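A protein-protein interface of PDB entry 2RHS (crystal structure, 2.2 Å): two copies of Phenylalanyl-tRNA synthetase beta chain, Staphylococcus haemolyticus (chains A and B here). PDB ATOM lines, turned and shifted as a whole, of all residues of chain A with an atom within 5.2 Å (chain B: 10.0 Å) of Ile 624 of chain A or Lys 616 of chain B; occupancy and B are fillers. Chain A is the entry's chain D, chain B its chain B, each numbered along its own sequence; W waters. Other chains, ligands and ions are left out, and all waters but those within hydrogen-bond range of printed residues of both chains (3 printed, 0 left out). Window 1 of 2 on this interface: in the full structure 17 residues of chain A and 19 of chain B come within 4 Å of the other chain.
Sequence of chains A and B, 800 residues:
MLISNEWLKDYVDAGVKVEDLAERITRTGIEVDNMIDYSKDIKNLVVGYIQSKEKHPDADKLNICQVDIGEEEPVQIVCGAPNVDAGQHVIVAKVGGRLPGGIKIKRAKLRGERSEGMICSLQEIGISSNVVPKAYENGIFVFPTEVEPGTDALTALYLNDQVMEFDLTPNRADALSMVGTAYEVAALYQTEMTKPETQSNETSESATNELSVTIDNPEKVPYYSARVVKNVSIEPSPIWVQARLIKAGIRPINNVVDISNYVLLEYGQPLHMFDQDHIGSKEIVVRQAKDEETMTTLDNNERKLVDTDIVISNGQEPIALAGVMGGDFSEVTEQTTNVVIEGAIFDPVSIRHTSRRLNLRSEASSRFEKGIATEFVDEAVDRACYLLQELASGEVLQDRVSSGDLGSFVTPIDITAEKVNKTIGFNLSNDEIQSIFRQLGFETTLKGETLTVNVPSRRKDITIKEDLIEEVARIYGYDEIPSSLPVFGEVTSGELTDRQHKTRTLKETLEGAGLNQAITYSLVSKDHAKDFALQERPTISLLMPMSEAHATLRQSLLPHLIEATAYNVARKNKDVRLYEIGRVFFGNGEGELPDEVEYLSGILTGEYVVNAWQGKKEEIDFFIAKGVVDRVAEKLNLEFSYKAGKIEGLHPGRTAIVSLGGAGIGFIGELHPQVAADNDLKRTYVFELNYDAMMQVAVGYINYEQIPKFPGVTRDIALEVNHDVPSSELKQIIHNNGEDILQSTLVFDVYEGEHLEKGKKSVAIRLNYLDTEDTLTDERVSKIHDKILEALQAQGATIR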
ATOM      1  N   LEU A 604     -18.802 -23.872 -36.831  1.00  0.00           N
ATOM      2  CA  LEU A 604     -18.876 -24.227 -35.420  1.00  0.00           C
ATOM      3  C   LEU A 604     -19.889 -25.341 -35.222  1.00  0.00           C
ATOM      4  O   LEU A 604     -21.016 -25.279 -35.737  1.00  0.00           O
ATOM      5  CB  LEU A 604     -19.362 -23.002 -34.603  1.00  0.00           C
ATOM      6  CG  LEU A 604     -18.558 -21.728 -34.889  1.00  0.00           C
ATOM      7  CD1 LEU A 604     -19.183 -20.455 -34.385  1.00  0.00           C
ATOM      8  CD2 LEU A 604     -17.226 -21.909 -34.225  1.00  0.00           C
ATOM      9  N   TYR A 608     -19.583 -25.887 -26.841  1.00  0.00           N
ATOM     10  CA  TYR A 608     -18.815 -24.704 -26.613  1.00  0.00           C
ATOM     11  C   TYR A 608     -18.187 -24.741 -25.226  1.00  0.00           C
ATOM     12  O   TYR A 608     -16.986 -24.496 -25.092  1.00  0.00           O
ATOM     13  CB  TYR A 608     -19.647 -23.441 -26.824  1.00  0.00           C
ATOM     14  CG  TYR A 608     -18.686 -22.284 -26.939  1.00  0.00           C
ATOM     15  CD1 TYR A 608     -18.793 -21.195 -26.102  1.00  0.00           C
ATOM     16  CD2 TYR A 608     -17.652 -22.297 -27.871  1.00  0.00           C
ATOM     17  CE1 TYR A 608     -17.892 -20.131 -26.176  1.00  0.00           C
ATOM     18  CE2 TYR A 608     -16.745 -21.240 -27.957  1.00  0.00           C
ATOM     19  CZ  TYR A 608     -16.873 -20.152 -27.091  1.00  0.00           C
ATOM     20  OH  TYR A 608     -16.024 -19.064 -27.127  1.00  0.00           O
ATOM     21  N   GLU A 618     -22.549 -26.720 -22.719  1.00  0.00           N
ATOM     22  CA  GLU A 618     -23.215 -25.746 -23.551  1.00  0.00           C
ATOM     23  C   GLU A 618     -23.010 -26.041 -25.024  1.00  0.00           C
ATOM     24  O   GLU A 618     -21.974 -25.696 -25.575  1.00  0.00           O
ATOM     25  CB  GLU A 618     -22.757 -24.334 -23.180  1.00  0.00           C
ATOM     26  CG  GLU A 618     -23.450 -23.262 -23.986  1.00  0.00           C
ATOM     27  CD  GLU A 618     -23.038 -21.875 -23.547  1.00  0.00           C
ATOM     28  OE1 GLU A 618     -22.109 -21.791 -22.716  1.00  0.00           O
ATOM     29  OE2 GLU A 618     -23.629 -20.881 -24.030  1.00  0.00           O
ATOM     30  N   GLU A 619     -24.015 -26.643 -25.645  1.00  0.00           N
ATOM     31  CA  GLU A 619     -24.065 -26.846 -27.095  1.00  0.00           C
ATOM     32  C   GLU A 619     -23.991 -25.568 -27.920  1.00  0.00           C
ATOM     33  O   GLU A 619     -24.684 -24.589 -27.652  1.00  0.00           O
ATOM     34  CB  GLU A 619     -25.331 -27.589 -27.544  1.00  0.00           C
ATOM     35  CG  GLU A 619     -25.573 -28.991 -26.961  1.00  0.00           C
ATOM     36  CD  GLU A 619     -24.498 -30.017 -27.327  1.00  0.00           C
ATOM     37  OE1 GLU A 619     -24.181 -30.197 -28.527  1.00  0.00           O
ATOM     38  OE2 GLU A 619     -23.959 -30.657 -26.394  1.00  0.00           O
ATOM     39  N   ILE A 620     -23.168 -25.593 -28.958  1.00  0.00           N
ATOM     40  CA  ILE A 620     -23.150 -24.501 -29.923  1.00  0.00           C
ATOM     41  C   ILE A 620     -24.499 -24.371 -30.622  1.00  0.00           C
ATOM     42  O   ILE A 620     -25.010 -25.344 -31.181  1.00  0.00           O
ATOM     43  CB  ILE A 620     -22.001 -24.661 -30.927  1.00  0.00           C
ATOM     44  CG1 ILE A 620     -20.696 -24.291 -30.220  1.00  0.00           C
ATOM     45  CG2 ILE A 620     -22.230 -23.752 -32.143  1.00  0.00           C
ATOM     46  CD1 ILE A 620     -19.439 -24.579 -31.051  1.00  0.00           C
ATOM     47  N   ASP A 621     -25.076 -23.173 -30.571  1.00  0.00           N
ATOM     48  CA  ASP A 621     -26.336 -22.884 -31.238  1.00  0.00           C
ATOM     49  C   ASP A 621     -26.179 -21.632 -32.087  1.00  0.00           C
ATOM     50  O   ASP A 621     -25.092 -21.072 -32.192  1.00  0.00           O
ATOM     51  CB  ASP A 621     -27.536 -22.827 -30.260  1.00  0.00           C
ATOM     52  CG  ASP A 621     -27.577 -21.539 -29.420  1.00  0.00           C
ATOM     53  OD1 ASP A 621     -26.538 -20.868 -29.237  1.00  0.00           O
ATOM     54  OD2 ASP A 621     -28.673 -21.180 -28.942  1.00  0.00           O
ATOM     55  N   PHE A 622     -27.260 -21.183 -32.710  1.00  0.00           N
ATOM     56  CA  PHE A 622     -27.142 -20.024 -33.568  1.00  0.00           C
ATOM     57  C   PHE A 622     -26.623 -18.852 -32.732  1.00  0.00           C
ATOM     58  O   PHE A 622     -25.779 -18.068 -33.157  1.00  0.00           O
ATOM     59  CB  PHE A 622     -28.529 -19.679 -34.092  1.00  0.00           C
ATOM     60  CG  PHE A 622     -28.553 -18.438 -34.923  1.00  0.00           C
ATOM     61  CD1 PHE A 622     -28.658 -17.192 -34.311  1.00  0.00           C
ATOM     62  CD2 PHE A 622     -28.453 -18.517 -36.306  1.00  0.00           C
ATOM     63  CE1 PHE A 622     -28.688 -16.035 -35.061  1.00  0.00           C
ATOM     64  CE2 PHE A 622     -28.496 -17.374 -37.061  1.00  0.00           C
ATOM     65  CZ  PHE A 622     -28.603 -16.126 -36.440  1.00  0.00           C
ATOM     66  N   PHE A 623     -27.121 -18.746 -31.508  1.00  0.00           N
ATOM     67  CA  PHE A 623     -26.824 -17.550 -30.750  1.00  0.00           C
ATOM     68  C   PHE A 623     -25.388 -17.477 -30.242  1.00  0.00           C
ATOM     69  O   PHE A 623     -24.932 -16.422 -29.832  1.00  0.00           O
ATOM     70  CB  PHE A 623     -27.933 -17.267 -29.739  1.00  0.00           C
ATOM     71  CG  PHE A 623     -29.250 -16.988 -30.415  1.00  0.00           C
ATOM     72  CD1 PHE A 623     -30.209 -17.986 -30.558  1.00  0.00           C
ATOM     73  CD2 PHE A 623     -29.506 -15.737 -30.967  1.00  0.00           C
ATOM     74  CE1 PHE A 623     -31.435 -17.725 -31.207  1.00  0.00           C
ATOM     75  CE2 PHE A 623     -30.706 -15.480 -31.625  1.00  0.00           C
ATOM     76  CZ  PHE A 623     -31.682 -16.460 -31.739  1.00  0.00           C
ATOM     77  N   ILE A 624     -24.666 -18.590 -30.279  1.00  0.00           N
ATOM     78  CA  ILE A 624     -23.298 -18.545 -29.821  1.00  0.00           C
ATOM     79  C   ILE A 624     -22.503 -18.191 -31.076  1.00  0.00           C
ATOM     80  O   ILE A 624     -21.548 -17.426 -31.050  1.00  0.00           O
ATOM     81  CB  ILE A 624     -22.828 -19.909 -29.305  1.00  0.00           C
ATOM     82  CG1 ILE A 624     -23.147 -20.091 -27.822  1.00  0.00           C
ATOM     83  CG2 ILE A 624     -21.322 -20.045 -29.552  1.00  0.00           C
ATOM     84  CD1 ILE A 624     -22.811 -21.498 -27.285  1.00  0.00           C
ATOM     85  N   ALA A 625     -22.921 -18.742 -32.207  1.00  0.00           N
ATOM     86  CA  ALA A 625     -22.371 -18.305 -33.488  1.00  0.00           C
ATOM     87  C   ALA A 625     -22.538 -16.798 -33.711  1.00  0.00           C
ATOM     88  O   ALA A 625     -21.660 -16.114 -34.253  1.00  0.00           O
ATOM     89  CB  ALA A 625     -22.931 -19.145 -34.651  1.00  0.00           C
ATOM     90  N   LYS A 626     -23.684 -16.282 -33.309  1.00  0.00           N
ATOM     91  CA  LYS A 626     -23.920 -14.842 -33.341  1.00  0.00           C
ATOM     92  C   LYS A 626     -22.965 -14.102 -32.423  1.00  0.00           C
ATOM     93  O   LYS A 626     -22.559 -12.975 -32.703  1.00  0.00           O
ATOM     94  CB  LYS A 626     -25.352 -14.545 -32.921  1.00  0.00           C
ATOM     95  CG  LYS A 626     -25.842 -13.242 -33.486  1.00  0.00           C
ATOM     96  CD  LYS A 626     -27.280 -12.977 -33.127  1.00  0.00           C
ATOM     97  CE  LYS A 626     -27.524 -11.484 -33.082  1.00  0.00           C
ATOM     98  NZ  LYS A 626     -28.941 -11.176 -32.776  1.00  0.00           N
ATOM     99  N   GLY A 627     -22.616 -14.764 -31.326  1.00  0.00           N
ATOM    100  CA  GLY A 627     -21.865 -14.189 -30.250  1.00  0.00           C
ATOM    101  C   GLY A 627     -20.441 -14.044 -30.703  1.00  0.00           C
ATOM    102  O   GLY A 627     -19.733 -13.159 -30.213  1.00  0.00           O
ATOM    103  N   VAL A 628     -20.023 -14.930 -31.608  1.00  0.00           N
ATOM    104  CA  VAL A 628     -18.684 -14.870 -32.209  1.00  0.00           C
ATOM    105  C   VAL A 628     -18.598 -13.725 -33.224  1.00  0.00           C
ATOM    106  O   VAL A 628     -17.560 -13.049 -33.313  1.00  0.00           O
ATOM    107  CB  VAL A 628     -18.346 -16.150 -33.042  1.00  0.00           C
ATOM    108  CG1 VAL A 628     -17.101 -15.919 -33.915  1.00  0.00           C
ATOM    109  CG2 VAL A 628     -18.230 -17.411 -32.182  1.00  0.00           C
ATOM    110  N   GLU B 607     -21.102 -12.964 -12.853  1.00  0.00           N
ATOM    111  CA  GLU B 607     -21.351 -13.934 -13.905  1.00  0.00           C
ATOM    112  C   GLU B 607     -20.266 -13.939 -14.951  1.00  0.00           C
ATOM    113  O   GLU B 607     -19.671 -12.901 -15.259  1.00  0.00           O
ATOM    114  CB  GLU B 607     -22.716 -13.749 -14.549  1.00  0.00           C
ATOM    115  CG  GLU B 607     -23.719 -14.721 -13.946  1.00  0.00           C
ATOM    116  CD  GLU B 607     -24.700 -13.971 -13.099  1.00  0.00           C
ATOM    117  OE1 GLU B 607     -25.410 -13.134 -13.702  1.00  0.00           O
ATOM    118  OE2 GLU B 607     -24.734 -14.215 -11.870  1.00  0.00           O
ATOM    119  N   TYR B 608     -20.021 -15.141 -15.456  1.00  0.00           N
ATOM    120  CA  TYR B 608     -19.062 -15.334 -16.512  1.00  0.00           C
ATOM    121  C   TYR B 608     -19.757 -15.299 -17.847  1.00  0.00           C
ATOM    122  O   TYR B 608     -19.279 -14.638 -18.780  1.00  0.00           O
ATOM    123  CB  TYR B 608     -18.334 -16.650 -16.361  1.00  0.00           C
ATOM    124  CG  TYR B 608     -17.108 -16.657 -17.244  1.00  0.00           C
ATOM    125  CD1 TYR B 608     -16.817 -17.760 -18.025  1.00  0.00           C
ATOM    126  CD2 TYR B 608     -16.251 -15.561 -17.307  1.00  0.00           C
ATOM    127  CE1 TYR B 608     -15.704 -17.792 -18.847  1.00  0.00           C
ATOM    128  CE2 TYR B 608     -15.111 -15.585 -18.127  1.00  0.00           C
ATOM    129  CZ  TYR B 608     -14.852 -16.709 -18.895  1.00  0.00           C
ATOM    130  OH  TYR B 608     -13.767 -16.807 -19.734  1.00  0.00           O
ATOM    131  N   VAL B 609     -20.871 -16.025 -17.898  1.00  0.00           N
ATOM    132  CA  VAL B 609     -21.727 -16.130 -19.068  1.00  0.00           C
ATOM    133  C   VAL B 609     -23.166 -15.852 -18.713  1.00  0.00           C
ATOM    134  O   VAL B 609     -23.744 -16.427 -17.786  1.00  0.00           O
ATOM    135  CB  VAL B 609     -21.713 -17.524 -19.725  1.00  0.00           C
ATOM    136  CG1 VAL B 609     -22.797 -17.595 -20.790  1.00  0.00           C
ATOM    137  CG2 VAL B 609     -20.338 -17.837 -20.293  1.00  0.00           C
ATOM    138  N   VAL B 610     -23.738 -14.944 -19.490  1.00  0.00           N
ATOM    139  CA  VAL B 610     -25.166 -14.726 -19.425  1.00  0.00           C
ATOM    140  C   VAL B 610     -25.783 -14.670 -20.825  1.00  0.00           C
ATOM    141  O   VAL B 610     -25.149 -14.185 -21.767  1.00  0.00           O
ATOM    142  CB  VAL B 610     -25.472 -13.451 -18.627  1.00  0.00           C
ATOM    143  CG1 VAL B 610     -25.333 -12.245 -19.534  1.00  0.00           C
ATOM    144  CG2 VAL B 610     -26.886 -13.548 -18.045  1.00  0.00           C
ATOM    145  N   ASN B 611     -27.015 -15.174 -20.939  1.00  0.00           N
ATOM    146  CA  ASN B 611     -27.947 -14.791 -21.994  1.00  0.00           C
ATOM    147  C   ASN B 611     -29.359 -15.117 -21.515  1.00  0.00           C
ATOM    148  O   ASN B 611     -29.799 -16.265 -21.558  1.00  0.00           O
ATOM    149  CB  ASN B 611     -27.622 -15.522 -23.323  1.00  0.00           C
ATOM    150  CG  ASN B 611     -27.960 -14.664 -24.517  1.00  0.00           C
ATOM    151  OD1 ASN B 611     -27.987 -13.437 -24.386  1.00  0.00           O
ATOM    152  ND2 ASN B 611     -28.207 -15.274 -25.671  1.00  0.00           N
ATOM    153  N   ALA B 612     -30.083 -14.114 -21.035  1.00  0.00           N
ATOM    154  CA  ALA B 612     -31.143 -14.380 -20.093  1.00  0.00           C
ATOM    155  C   ALA B 612     -32.350 -14.971 -20.808  1.00  0.00           C
ATOM    156  O   ALA B 612     -32.994 -15.871 -20.268  1.00  0.00           O
ATOM    157  CB  ALA B 612     -31.510 -13.103 -19.269  1.00  0.00           C
ATOM    158  N   TRP B 613     -32.661 -14.488 -22.011  1.00  0.00           N
ATOM    159  CA  TRP B 613     -33.813 -15.005 -22.759  1.00  0.00           C
ATOM    160  C   TRP B 613     -33.674 -16.517 -22.968  1.00  0.00           C
ATOM    161  O   TRP B 613     -34.672 -17.237 -23.110  1.00  0.00           O
ATOM    162  CB  TRP B 613     -34.027 -14.237 -24.075  1.00  0.00           C
ATOM    163  CG  TRP B 613     -33.059 -14.594 -25.181  1.00  0.00           C
ATOM    164  CD1 TRP B 613     -31.831 -14.054 -25.410  1.00  0.00           C
ATOM    165  CD2 TRP B 613     -33.258 -15.574 -26.204  1.00  0.00           C
ATOM    166  NE1 TRP B 613     -31.246 -14.639 -26.516  1.00  0.00           N
ATOM    167  CE2 TRP B 613     -32.105 -15.577 -27.019  1.00  0.00           C
ATOM    168  CE3 TRP B 613     -34.292 -16.456 -26.509  1.00  0.00           C
ATOM    169  CZ2 TRP B 613     -31.960 -16.431 -28.113  1.00  0.00           C
ATOM    170  CZ3 TRP B 613     -34.138 -17.311 -27.595  1.00  0.00           C
ATOM    171  CH2 TRP B 613     -32.987 -17.283 -28.381  1.00  0.00           C
ATOM    172  N   GLN B 614     -32.425 -16.987 -22.960  1.00  0.00           N
ATOM    173  CA  GLN B 614     -32.124 -18.400 -23.149  1.00  0.00           C
ATOM    174  C   GLN B 614     -31.919 -19.074 -21.796  1.00  0.00           C
ATOM    175  O   GLN B 614     -31.702 -20.284 -21.766  1.00  0.00           O
ATOM    176  CB  GLN B 614     -30.824 -18.582 -23.946  1.00  0.00           C
ATOM    177  CG  GLN B 614     -30.915 -18.132 -25.411  1.00  0.00           C
ATOM    178  CD  GLN B 614     -29.786 -18.658 -26.240  1.00  0.00           C
ATOM    179  OE1 GLN B 614     -28.647 -18.221 -26.079  1.00  0.00           O
ATOM    180  NE2 GLN B 614     -30.085 -19.602 -27.135  1.00  0.00           N
ATOM    181  N   GLY B 615     -31.952 -18.309 -20.705  1.00  0.00           N
ATOM    182  CA  GLY B 615     -31.751 -18.896 -19.375  1.00  0.00           C
ATOM    183  C   GLY B 615     -30.312 -19.290 -19.084  1.00  0.00           C
ATOM    184  O   GLY B 615     -30.028 -20.142 -18.248  1.00  0.00           O
ATOM    185  N   LYS B 616     -29.368 -18.664 -19.774  1.00  0.00           N
ATOM    186  CA  LYS B 616     -27.974 -18.947 -19.487  1.00  0.00           C
ATOM    187  C   LYS B 616     -27.437 -17.920 -18.511  1.00  0.00           C
ATOM    188  O   LYS B 616     -27.548 -16.695 -18.694  1.00  0.00           O
ATOM    189  CB  LYS B 616     -27.156 -18.977 -20.760  1.00  0.00           C
ATOM    190  CG  LYS B 616     -27.576 -20.080 -21.720  1.00  0.00           C
ATOM    191  CD  LYS B 616     -26.710 -19.952 -23.003  1.00  0.00           C
ATOM    192  CE  LYS B 616     -26.866 -21.175 -23.936  1.00  0.00           C
ATOM    193  NZ  LYS B 616     -25.689 -21.288 -24.845  1.00  0.00           N
ATOM    194  N   LYS B 617     -26.846 -18.469 -17.457  1.00  0.00           N
ATOM    195  CA  LYS B 617     -26.352 -17.683 -16.360  1.00  0.00           C
ATOM    196  C   LYS B 617     -25.320 -18.610 -15.737  1.00  0.00           C
ATOM    197  O   LYS B 617     -25.676 -19.502 -14.979  1.00  0.00           O
ATOM    198  CB  LYS B 617     -27.480 -17.405 -15.365  1.00  0.00           C
ATOM    199  CG  LYS B 617     -27.152 -16.331 -14.333  1.00  0.00           C
ATOM    200  CD  LYS B 617     -28.320 -16.025 -13.385  1.00  0.00           C
ATOM    201  CE  LYS B 617     -27.944 -14.851 -12.511  1.00  0.00           C
ATOM    202  NZ  LYS B 617     -29.087 -14.340 -11.719  1.00  0.00           N
ATOM    203  N   GLU B 618     -24.045 -18.405 -16.045  1.00  0.00           N
ATOM    204  CA  GLU B 618     -23.033 -19.253 -15.452  1.00  0.00           C
ATOM    205  C   GLU B 618     -22.129 -18.435 -14.543  1.00  0.00           C
ATOM    206  O   GLU B 618     -21.282 -17.656 -14.987  1.00  0.00           O
ATOM    207  CB  GLU B 618     -22.296 -20.013 -16.551  1.00  0.00           C
ATOM    208  CG  GLU B 618     -20.985 -20.641 -16.147  1.00  0.00           C
ATOM    209  CD  GLU B 618     -20.210 -21.105 -17.364  1.00  0.00           C
ATOM    210  OE1 GLU B 618     -20.576 -20.680 -18.478  1.00  0.00           O
ATOM    211  OE2 GLU B 618     -19.262 -21.895 -17.220  1.00  0.00           O
ATOM    212  N   GLU B 619     -22.343 -18.629 -13.249  1.00  0.00           N
ATOM    213  CA  GLU B 619     -21.677 -17.902 -12.174  1.00  0.00           C
ATOM    214  C   GLU B 619     -20.200 -18.243 -12.099  1.00  0.00           C
ATOM    215  O   GLU B 619     -19.777 -19.377 -12.318  1.00  0.00           O
ATOM    216  CB  GLU B 619     -22.341 -18.241 -10.842  1.00  0.00           C
ATOM    217  CG  GLU B 619     -22.209 -17.162  -9.770  1.00  0.00           C
ATOM    218  CD  GLU B 619     -22.806 -17.622  -8.438  1.00  0.00           C
ATOM    219  OE1 GLU B 619     -24.009 -17.989  -8.443  1.00  0.00           O
ATOM    220  OE2 GLU B 619     -22.077 -17.622  -7.413  1.00  0.00           O
HETATM  221  O   HOH W   1     -26.458 -23.642 -26.016  1.00  0.00           O
HETATM  222  O   HOH W   2     -26.419 -19.602 -26.818  1.00  0.00           O
HETATM  223  O   HOH W   3     -22.169 -21.580 -20.203  1.00  0.00           O
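The side-chain amide nitrogen (ND2) of Asn 611 of chain B lies close to the indole nitrogen (NE1) of Trp 613 of chain B, at 3.2 Å. ND2 of Asn 611 of chain B lies within hydrogen-bond range of OE1 of Gln 614 of chain B. N of Asn 611 of chain B lies within hydrogen-bond range of O of Lys 616 of chain B. The backbone NH of Tyr 608 of chain A lies within hydrogen-bond range of the backbone carbonyl oxygen of Glu 618 of chain A, at 2.7 Å. N of Phe 623 of chain A lies close to OD1 of Asp 621 of chain A, 3.2 Å away. N of Ile 624 of chain A sits at hydrogen-bond distance from OD1 of Asp 621 of chain A, at 3.1 Å.
Water W3 bridges OE1 of Glu 618 of chain B (2.5 Å) and OE1 of Glu 618 of chain A (2.5 Å). Water W1 bridges O of Glu 619 of chain A (2.6 Å) and NZ of Lys 616 of chain B (2.7 Å). Water W2 lies within hydrogen-bond range of NZ of Lys 616 of chain B, OE1 of Gln 614 of chain B and OD1 of Asp 621 of chain A.
OD2 of Asp 621 of chain A lies within hydrogen-bond range of NE2 of Gln 614 of chain B, 2.8 Å away. The side-chain amino group (NZ) of Lys 616 of chain B lies close to the side-chain carboxylate (OE2) of Glu 618 of chain A, 2.3 Å away.
Among the printed residues, pairs that only touch across the chains: Phe 623 of chain A with Trp 613 of chain B (3.3 Å), Phe 623 of chain A with Gln 614 of chain B (3.8 Å) and Ile 624 of chain A with Lys 616 of chain B (3.8 Å).
Ile 624 of chain A touches one residue of chain B. Lys 616 of chain B touches just these residues of chain A: Glu 618 and Ile 624. No residue of chain B comes within 4 Å of Ile 620 of chain A. No residue of chain B comes within 4 Å of Gly 627 of chain A. Of the printed residues of chain B, Glu 618 of chain A touches Lys 616. Of the printed residues of chain A, Gln 614 of chain B touches Asp 621 (2.8 Å) and Phe 623 (3.8 Å). Of the printed residues of chain A, Trp 613 of chain B touches Phe 623 (3.3 Å). Of the printed residues of chain B, Phe 623 of chain A touches Trp 613 and Gln 614. Glu 619 of chain A touches none of the printed residues of chain B. The nearest residue of chain B that does not touch Ile 624 of chain A is Gln 614 of chain B (5.8 Å). The nearest residue of chain A that does not touch Lys 616 of chain B is Glu 619 of chain A (4.4 Å). The nearest printed residue of chain A that does not touch Gln 614 of chain B is Ile 624 of chain A (5.8 Å).
Positions printed for both chains: 608, 618 and 619. Of the 5 pairs that touch across the chains among the printed residues, none has its exchanged pair printed and touching as well.
Of the 13 printed residues of chain B, 3 touch a printed residue of chain A. Along chain B the printed residues that touch a printed residue of chain A span positions 613 to 616. Among the printed residues, 5 pairs touch across the chains.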
